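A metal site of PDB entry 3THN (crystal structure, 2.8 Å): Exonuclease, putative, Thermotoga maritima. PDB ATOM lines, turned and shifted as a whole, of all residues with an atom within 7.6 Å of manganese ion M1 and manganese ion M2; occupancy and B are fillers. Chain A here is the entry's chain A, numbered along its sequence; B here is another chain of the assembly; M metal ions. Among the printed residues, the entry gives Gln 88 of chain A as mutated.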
ATOM      1  N   SER A   7     -11.736  -5.293  13.328  1.00  0.00           N
ATOM      2  CA  SER A   7     -12.389  -5.592  12.065  1.00  0.00           C
ATOM      3  C   SER A   7     -12.975  -6.986  12.016  1.00  0.00           C
ATOM      4  O   SER A   7     -12.683  -7.821  12.855  1.00  0.00           O
ATOM      5  CB  SER A   7     -11.352  -5.445  10.944  1.00  0.00           C
ATOM      6  OG  SER A   7     -11.974  -5.053   9.737  1.00  0.00           O
ATOM      7  N   ASP A   8     -13.792  -7.215  10.995  1.00  0.00           N
ATOM      8  CA  ASP A   8     -14.131  -8.572  10.589  1.00  0.00           C
ATOM      9  C   ASP A   8     -14.683  -9.386  11.748  1.00  0.00           C
ATOM     10  O   ASP A   8     -14.211 -10.491  12.019  1.00  0.00           O
ATOM     11  CB  ASP A   8     -12.904  -9.258   9.978  1.00  0.00           C
ATOM     12  CG  ASP A   8     -12.423  -8.572   8.698  1.00  0.00           C
ATOM     13  OD1 ASP A   8     -11.640  -7.609   8.811  1.00  0.00           O
ATOM     14  OD2 ASP A   8     -12.819  -9.008   7.594  1.00  0.00           O
ATOM     15  N   TRP A   9     -15.675  -8.830  12.418  1.00  0.00           N
ATOM     16  CA  TRP A   9     -16.265  -9.461  13.585  1.00  0.00           C
ATOM     17  C   TRP A   9     -17.107 -10.669  13.198  1.00  0.00           C
ATOM     18  O   TRP A   9     -17.079 -11.701  13.857  1.00  0.00           O
ATOM     19  CB  TRP A   9     -17.151  -8.469  14.305  1.00  0.00           C
ATOM     20  CG  TRP A   9     -16.425  -7.343  14.951  1.00  0.00           C
ATOM     21  CD1 TRP A   9     -15.075  -7.199  15.096  1.00  0.00           C
ATOM     22  CD2 TRP A   9     -17.030  -6.200  15.564  1.00  0.00           C
ATOM     23  NE1 TRP A   9     -14.804  -6.022  15.767  1.00  0.00           N
ATOM     24  CE2 TRP A   9     -15.983  -5.390  16.062  1.00  0.00           C
ATOM     25  CE3 TRP A   9     -18.345  -5.780  15.745  1.00  0.00           C
ATOM     26  CZ2 TRP A   9     -16.227  -4.191  16.712  1.00  0.00           C
ATOM     27  CZ3 TRP A   9     -18.579  -4.585  16.396  1.00  0.00           C
ATOM     28  CH2 TRP A   9     -17.520  -3.805  16.874  1.00  0.00           C
ATOM     29  N   HIS A  10     -17.870 -10.510  12.121  1.00  0.00           N
ATOM     30  CA  HIS A  10     -18.810 -11.534  11.685  1.00  0.00           C
ATOM     31  C   HIS A  10     -19.863 -11.879  12.748  1.00  0.00           C
ATOM     32  O   HIS A  10     -20.142 -13.050  12.987  1.00  0.00           O
ATOM     33  CB  HIS A  10     -18.079 -12.789  11.245  1.00  0.00           C
ATOM     34  CG  HIS A  10     -17.368 -12.637   9.930  1.00  0.00           C
ATOM     35  ND1 HIS A  10     -17.818 -13.228   8.776  1.00  0.00           N
ATOM     36  CD2 HIS A  10     -16.256 -11.948   9.596  1.00  0.00           C
ATOM     37  CE1 HIS A  10     -17.010 -12.921   7.774  1.00  0.00           C
ATOM     38  NE2 HIS A  10     -16.048 -12.143   8.252  1.00  0.00           N
ATOM     39  N   THR A  50     -13.100  -1.455  10.339  1.00  0.00           N
ATOM     40  CA  THR A  50     -12.961  -1.573   8.878  1.00  0.00           C
ATOM     41  C   THR A  50     -13.818  -2.655   8.208  1.00  0.00           C
ATOM     42  O   THR A  50     -13.400  -3.238   7.221  1.00  0.00           O
ATOM     43  CB  THR A  50     -11.485  -1.707   8.438  1.00  0.00           C
ATOM     44  OG1 THR A  50     -10.744  -2.458   9.412  1.00  0.00           O
ATOM     45  CG2 THR A  50     -10.841  -0.340   8.304  1.00  0.00           C
ATOM     46  N   GLY A  51     -15.008  -2.913   8.736  1.00  0.00           N
ATOM     47  CA  GLY A  51     -16.019  -3.625   7.977  1.00  0.00           C
ATOM     48  C   GLY A  51     -16.181  -5.101   8.267  1.00  0.00           C
ATOM     49  O   GLY A  51     -15.376  -5.683   8.981  1.00  0.00           O
ATOM     50  N   ASP A  52     -17.205  -5.704   7.656  1.00  0.00           N
ATOM     51  CA  ASP A  52     -17.622  -7.094   7.921  1.00  0.00           C
ATOM     52  C   ASP A  52     -17.943  -7.314   9.397  1.00  0.00           C
ATOM     53  O   ASP A  52     -17.613  -8.360   9.966  1.00  0.00           O
ATOM     54  CB  ASP A  52     -16.583  -8.102   7.471  1.00  0.00           C
ATOM     55  CG  ASP A  52     -16.535  -8.273   5.968  1.00  0.00           C
ATOM     56  OD1 ASP A  52     -17.461  -7.778   5.281  1.00  0.00           O
ATOM     57  OD2 ASP A  52     -15.561  -8.894   5.478  1.00  0.00           O
ATOM     58  N   LEU A  53     -18.588  -6.332  10.014  1.00  0.00           N
ATOM     59  CA  LEU A  53     -19.007  -6.462  11.393  1.00  0.00           C
ATOM     60  C   LEU A  53     -20.125  -7.490  11.540  1.00  0.00           C
ATOM     61  O   LEU A  53     -20.186  -8.236  12.519  1.00  0.00           O
ATOM     62  CB  LEU A  53     -19.465  -5.092  11.907  1.00  0.00           C
ATOM     63  CG  LEU A  53     -18.426  -4.018  11.618  1.00  0.00           C
ATOM     64  CD1 LEU A  53     -18.877  -2.706  12.178  1.00  0.00           C
ATOM     65  CD2 LEU A  53     -17.071  -4.418  12.210  1.00  0.00           C
ATOM     66  N   LEU A  54     -21.019  -7.515  10.559  1.00  0.00           N
ATOM     67  CA  LEU A  54     -22.059  -8.526  10.489  1.00  0.00           C
ATOM     68  C   LEU A  54     -21.648  -9.632   9.540  1.00  0.00           C
ATOM     69  O   LEU A  54     -20.786  -9.439   8.670  1.00  0.00           O
ATOM     70  CB  LEU A  54     -23.372  -7.935  10.002  1.00  0.00           C
ATOM     71  CG  LEU A  54     -24.219  -7.179  11.002  1.00  0.00           C
ATOM     72  CD1 LEU A  54     -25.396  -6.566  10.269  1.00  0.00           C
ATOM     73  CD2 LEU A  54     -24.684  -8.126  12.063  1.00  0.00           C
ATOM     74  N   PRO A  85     -18.147   0.034   6.301  1.00  0.00           N
ATOM     75  CA  PRO A  85     -18.749  -1.295   6.098  1.00  0.00           C
ATOM     76  C   PRO A  85     -18.089  -2.041   4.940  1.00  0.00           C
ATOM     77  O   PRO A  85     -17.568  -1.399   4.024  1.00  0.00           O
ATOM     78  CB  PRO A  85     -20.217  -0.990   5.794  1.00  0.00           C
ATOM     79  CG  PRO A  85     -20.301   0.509   5.611  1.00  0.00           C
ATOM     80  CD  PRO A  85     -19.155   1.097   6.363  1.00  0.00           C
ATOM     81  N   GLY A  86     -18.083  -3.376   5.004  1.00  0.00           N
ATOM     82  CA  GLY A  86     -17.495  -4.228   3.974  1.00  0.00           C
ATOM     83  C   GLY A  86     -18.518  -4.918   3.079  1.00  0.00           C
ATOM     84  O   GLY A  86     -19.703  -4.545   3.041  1.00  0.00           O
ATOM     85  N   ASN A  87     -18.050  -5.938   2.351  1.00  0.00           N
ATOM     86  CA  ASN A  87     -18.895  -6.651   1.399  1.00  0.00           C
ATOM     87  C   ASN A  87     -20.020  -7.410   2.088  1.00  0.00           C
ATOM     88  O   ASN A  87     -21.122  -7.462   1.564  1.00  0.00           O
ATOM     89  CB  ASN A  87     -18.072  -7.612   0.534  1.00  0.00           C
ATOM     90  CG  ASN A  87     -17.011  -8.351   1.323  1.00  0.00           C
ATOM     91  OD1 ASN A  87     -16.149  -7.717   1.962  1.00  0.00           O
ATOM     92  ND2 ASN A  87     -17.076  -9.686   1.338  1.00  0.00           N
ATOM     93  N   GLN A  88     -19.747  -7.967   3.261  1.00  0.00           N
ATOM     94  CA  GLN A  88     -20.715  -8.823   3.947  1.00  0.00           C
ATOM     95  C   GLN A  88     -21.517  -8.127   5.043  1.00  0.00           C
ATOM     96  O   GLN A  88     -22.166  -8.791   5.854  1.00  0.00           O
ATOM     97  CB  GLN A  88     -20.032 -10.034   4.565  1.00  0.00           C
ATOM     98  CG  GLN A  88     -19.108 -10.746   3.611  1.00  0.00           C
ATOM     99  CD  GLN A  88     -18.281 -11.783   4.319  1.00  0.00           C
ATOM    100  OE1 GLN A  88     -18.769 -12.451   5.242  1.00  0.00           O
ATOM    101  NE2 GLN A  88     -17.002 -11.917   3.922  1.00  0.00           N
ATOM    102  N   ASP A  89     -21.468  -6.815   5.114  1.00  0.00           N
ATOM    103  CA  ASP A  89     -22.377  -6.130   6.016  1.00  0.00           C
ATOM    104  C   ASP A  89     -23.709  -5.916   5.336  1.00  0.00           C
ATOM    105  O   ASP A  89     -23.783  -5.451   4.194  1.00  0.00           O
ATOM    106  CB  ASP A  89     -21.778  -4.811   6.489  1.00  0.00           C
ATOM    107  CG  ASP A  89     -20.636  -5.016   7.437  1.00  0.00           C
ATOM    108  OD1 ASP A  89     -19.602  -4.325   7.283  1.00  0.00           O
ATOM    109  OD2 ASP A  89     -20.777  -5.875   8.344  1.00  0.00           O
ATOM    110  N   TYR A 133     -14.913  -1.793  -0.513  1.00  0.00           N
ATOM    111  CA  TYR A 133     -14.709  -3.012  -1.290  1.00  0.00           C
ATOM    112  C   TYR A 133     -14.976  -2.788  -2.766  1.00  0.00           C
ATOM    113  O   TYR A 133     -16.032  -2.284  -3.130  1.00  0.00           O
ATOM    114  CB  TYR A 133     -15.633  -4.128  -0.771  1.00  0.00           C
ATOM    115  CG  TYR A 133     -15.347  -5.529  -1.293  1.00  0.00           C
ATOM    116  CD1 TYR A 133     -14.166  -6.193  -0.975  1.00  0.00           C
ATOM    117  CD2 TYR A 133     -16.299  -6.201  -2.056  1.00  0.00           C
ATOM    118  CE1 TYR A 133     -13.922  -7.492  -1.434  1.00  0.00           C
ATOM    119  CE2 TYR A 133     -16.062  -7.494  -2.526  1.00  0.00           C
ATOM    120  CZ  TYR A 133     -14.883  -8.133  -2.209  1.00  0.00           C
ATOM    121  OH  TYR A 133     -14.673  -9.410  -2.667  1.00  0.00           O
ATOM    122  N   HIS A 174     -11.208  -1.785   2.451  1.00  0.00           N
ATOM    123  CA  HIS A 174     -11.758  -3.113   2.655  1.00  0.00           C
ATOM    124  C   HIS A 174     -11.547  -3.886   1.361  1.00  0.00           C
ATOM    125  O   HIS A 174     -12.309  -3.726   0.405  1.00  0.00           O
ATOM    126  CB  HIS A 174     -13.234  -3.048   3.045  1.00  0.00           C
ATOM    127  CG  HIS A 174     -13.775  -4.343   3.571  1.00  0.00           C
ATOM    128  ND1 HIS A 174     -13.804  -4.638   4.920  1.00  0.00           N
ATOM    129  CD2 HIS A 174     -14.290  -5.420   2.937  1.00  0.00           C
ATOM    130  CE1 HIS A 174     -14.317  -5.847   5.090  1.00  0.00           C
ATOM    131  NE2 HIS A 174     -14.611  -6.347   3.897  1.00  0.00           N
ATOM    132  N   PHE A 175     -10.476  -4.689   1.338  1.00  0.00           N
ATOM    133  CA  PHE A 175     -10.111  -5.458   0.147  1.00  0.00           C
ATOM    134  C   PHE A 175      -8.970  -6.440   0.409  1.00  0.00           C
ATOM    135  O   PHE A 175      -8.421  -6.479   1.506  1.00  0.00           O
ATOM    136  CB  PHE A 175      -9.719  -4.526  -1.003  1.00  0.00           C
ATOM    137  CG  PHE A 175      -8.718  -3.464  -0.616  1.00  0.00           C
ATOM    138  CD1 PHE A 175      -7.374  -3.771  -0.516  1.00  0.00           C
ATOM    139  CD2 PHE A 175      -9.124  -2.157  -0.377  1.00  0.00           C
ATOM    140  CE1 PHE A 175      -6.435  -2.798  -0.166  1.00  0.00           C
ATOM    141  CE2 PHE A 175      -8.195  -1.181  -0.027  1.00  0.00           C
ATOM    142  CZ  PHE A 175      -6.837  -1.506   0.079  1.00  0.00           C
ATOM    143  N   THR A 176      -8.633  -7.242  -0.592  1.00  0.00           N
ATOM    144  CA  THR A 176      -7.446  -8.084  -0.517  1.00  0.00           C
ATOM    145  C   THR A 176      -6.296  -7.444  -1.267  1.00  0.00           C
ATOM    146  O   THR A 176      -6.482  -6.955  -2.381  1.00  0.00           O
ATOM    147  CB  THR A 176      -7.669  -9.463  -1.135  1.00  0.00           C
ATOM    148  OG1 THR A 176      -9.052  -9.813  -1.038  1.00  0.00           O
ATOM    149  CG2 THR A 176      -6.806 -10.489  -0.427  1.00  0.00           C
ATOM    150  N   GLU A 191     -11.485 -12.134  -6.901  1.00  0.00           N
ATOM    151  CA  GLU A 191     -11.659 -10.798  -6.346  1.00  0.00           C
ATOM    152  C   GLU A 191     -10.895  -9.809  -7.192  1.00  0.00           C
ATOM    153  O   GLU A 191      -9.955 -10.199  -7.907  1.00  0.00           O
ATOM    154  CB  GLU A 191     -11.089 -10.714  -4.933  1.00  0.00           C
ATOM    155  CG  GLU A 191     -11.636 -11.696  -3.936  1.00  0.00           C
ATOM    156  CD  GLU A 191     -11.810 -11.067  -2.581  1.00  0.00           C
ATOM    157  OE1 GLU A 191     -11.722  -9.823  -2.517  1.00  0.00           O
ATOM    158  OE2 GLU A 191     -12.047 -11.794  -1.590  1.00  0.00           O
ATOM    159  N   GLY A 209      -9.457  -4.059   6.212  1.00  0.00           N
ATOM    160  CA  GLY A 209     -10.276  -5.167   6.659  1.00  0.00           C
ATOM    161  C   GLY A 209     -10.584  -6.043   5.470  1.00  0.00           C
ATOM    162  O   GLY A 209     -10.433  -5.603   4.338  1.00  0.00           O
ATOM    163  N   HIS A 210     -10.970  -7.291   5.753  1.00  0.00           N
ATOM    164  CA  HIS A 210     -11.548  -8.259   4.808  1.00  0.00           C
ATOM    165  C   HIS A 210     -10.795  -9.582   4.970  1.00  0.00           C
ATOM    166  O   HIS A 210     -11.332 -10.676   4.786  1.00  0.00           O
ATOM    167  CB  HIS A 210     -11.490  -7.765   3.357  1.00  0.00           C
ATOM    168  CG  HIS A 210     -11.947  -8.773   2.335  1.00  0.00           C
ATOM    169  ND1 HIS A 210     -13.270  -9.084   2.132  1.00  0.00           N
ATOM    170  CD2 HIS A 210     -11.241  -9.509   1.443  1.00  0.00           C
ATOM    171  CE1 HIS A 210     -13.370  -9.986   1.167  1.00  0.00           C
ATOM    172  NE2 HIS A 210     -12.151 -10.257   0.737  1.00  0.00           N
ATOM    173  N   ILE A 211      -9.542  -9.446   5.353  1.00  0.00           N
ATOM    174  CA  ILE A 211      -8.692 -10.583   5.566  1.00  0.00           C
ATOM    175  C   ILE A 211      -8.779 -10.950   7.037  1.00  0.00           C
ATOM    176  O   ILE A 211      -8.795 -10.066   7.903  1.00  0.00           O
ATOM    177  CB  ILE A 211      -7.256 -10.264   5.074  1.00  0.00           C
ATOM    178  CG1 ILE A 211      -7.272 -10.240   3.544  1.00  0.00           C
ATOM    179  CG2 ILE A 211      -6.266 -11.283   5.573  1.00  0.00           C
ATOM    180  CD1 ILE A 211      -7.909 -11.471   2.910  1.00  0.00           C
ATOM    181  N   HIS A 212      -8.874 -12.250   7.323  1.00  0.00           N
ATOM    182  CA  HIS A 212      -9.149 -12.743   8.681  1.00  0.00           C
ATOM    183  C   HIS A 212      -7.910 -12.972   9.510  1.00  0.00           C
ATOM    184  O   HIS A 212      -8.012 -13.178  10.723  1.00  0.00           O
ATOM    185  CB  HIS A 212      -9.959 -14.046   8.649  1.00  0.00           C
ATOM    186  CG  HIS A 212     -11.243 -13.944   7.902  1.00  0.00           C
ATOM    187  ND1 HIS A 212     -12.002 -15.038   7.557  1.00  0.00           N
ATOM    188  CD2 HIS A 212     -11.900 -12.866   7.403  1.00  0.00           C
ATOM    189  CE1 HIS A 212     -13.064 -14.648   6.874  1.00  0.00           C
ATOM    190  NE2 HIS A 212     -13.030 -13.330   6.768  1.00  0.00           N
ATOM    191  N   GLY A 227      -7.311  -8.739  11.607  1.00  0.00           N
ATOM    192  CA  GLY A 227      -7.832 -10.098  11.586  1.00  0.00           C
ATOM    193  C   GLY A 227      -9.175 -10.271  12.266  1.00  0.00           C
ATOM    194  O   GLY A 227      -9.725  -9.310  12.809  1.00  0.00           O
ATOM    195  N   SER A 228      -9.717 -11.489  12.229  1.00  0.00           N
ATOM    196  CA  SER A 228     -10.951 -11.821  12.948  1.00  0.00           C
ATOM    197  C   SER A 228     -10.685 -11.813  14.449  1.00  0.00           C
ATOM    198  O   SER A 228      -9.573 -11.611  14.890  1.00  0.00           O
ATOM    199  CB  SER A 228     -11.423 -13.206  12.599  1.00  0.00           C
ATOM    200  OG  SER A 228     -11.048 -13.573  11.304  1.00  0.00           O
ATOM    201  N   ILE A 232     -12.968 -18.851  12.020  1.00  0.00           N
ATOM    202  CA  ILE A 232     -14.271 -19.114  11.402  1.00  0.00           C
ATOM    203  C   ILE A 232     -14.426 -20.532  10.817  1.00  0.00           C
ATOM    204  O   ILE A 232     -15.418 -21.192  11.124  1.00  0.00           O
ATOM    205  CB  ILE A 232     -14.604 -18.041  10.328  1.00  0.00           C
ATOM    206  CG1 ILE A 232     -14.978 -16.723  11.017  1.00  0.00           C
ATOM    207  CG2 ILE A 232     -15.747 -18.501   9.472  1.00  0.00           C
ATOM    208  CD1 ILE A 232     -14.547 -15.465  10.233  1.00  0.00           C
ATOM    209  N   ALA B 181      -6.567 -15.219   4.482  1.00  0.00           N
ATOM    210  CA  ALA B 181      -7.951 -15.636   4.279  1.00  0.00           C
ATOM    211  C   ALA B 181      -8.800 -14.537   4.917  1.00  0.00           C
ATOM    212  O   ALA B 181      -8.282 -13.784   5.723  1.00  0.00           O
ATOM    213  CB  ALA B 181      -8.198 -16.899   5.016  1.00  0.00           C
ATOM    214  N   GLY B 182     -10.082 -14.425   4.592  1.00  0.00           N
ATOM    215  CA  GLY B 182     -10.738 -15.143   3.539  1.00  0.00           C
ATOM    216  C   GLY B 182     -10.933 -14.279   2.295  1.00  0.00           C
ATOM    217  O   GLY B 182     -11.872 -13.472   2.163  1.00  0.00           O
HETATM  218 MN    MN M   1     -14.920  -8.433   3.423  1.00  0.00          MN
HETATM  219 MN    MN M   2     -14.244 -10.726   6.745  1.00  0.00          MN
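ND2 of Asn 87 lies close to NE2 of Gln 88, 3.4 Å away. The backbone carbonyl oxygen of Thr 50 lies within hydrogen-bond range of a ring nitrogen (ND1) of His 174, 2.7 Å away. The side-chain carboxylate of Asp 8 sits at hydrogen-bond distance from the backbone NH of His 210 (3.1 Å). A ring nitrogen (NE2) of His 210 sits at hydrogen-bond distance from the side-chain carboxylate (OE2) of Glu 191 (2.8 Å). N of Gln 88 sits at hydrogen-bond distance from OD1 of Asp 52 (3.1 Å). O of Asp 52 sits at hydrogen-bond distance from N of Trp 9. OD1 of Asp 8 sits at hydrogen-bond distance from OG of Ser 7. The backbone NH (N) of Ser 228 is in hydrogen-bond range of the backbone carbonyl oxygen (O) of His 212 (2.8 Å).
Of the 28 residues printed, 5 come within 4 Å of manganese ion M2. The nearest printed residue that does not touch manganese ion M2 is Gln 88 (4.1 Å).
The side-chain amide oxygen (OD1) of Asn 87 is bound to manganese ion M1 (2.0 Å). NE2 of His 174 is bound to manganese ion M1 (2.2 Å). ND1 of His 210 is bound to manganese ion M1, 2.2 Å away. Manganese ion M1 is bound by the side-chain carboxylate (OD2) of Asp 52, 2.2 Å away.
Manganese ion M2 is bound by the side-chain carboxylate of Asp 8 (2.4 Å) and the side-chain carboxylate of Asp 52 (2.6 Å). Manganese ion M2 has two donor atoms within binding distance. Slightly farther from manganese ion M2 lies a ring nitrogen (NE2) of His 10 (2.7 Å). Slightly farther from manganese ion M2 lies NE2 of His 212 (2.9 Å).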
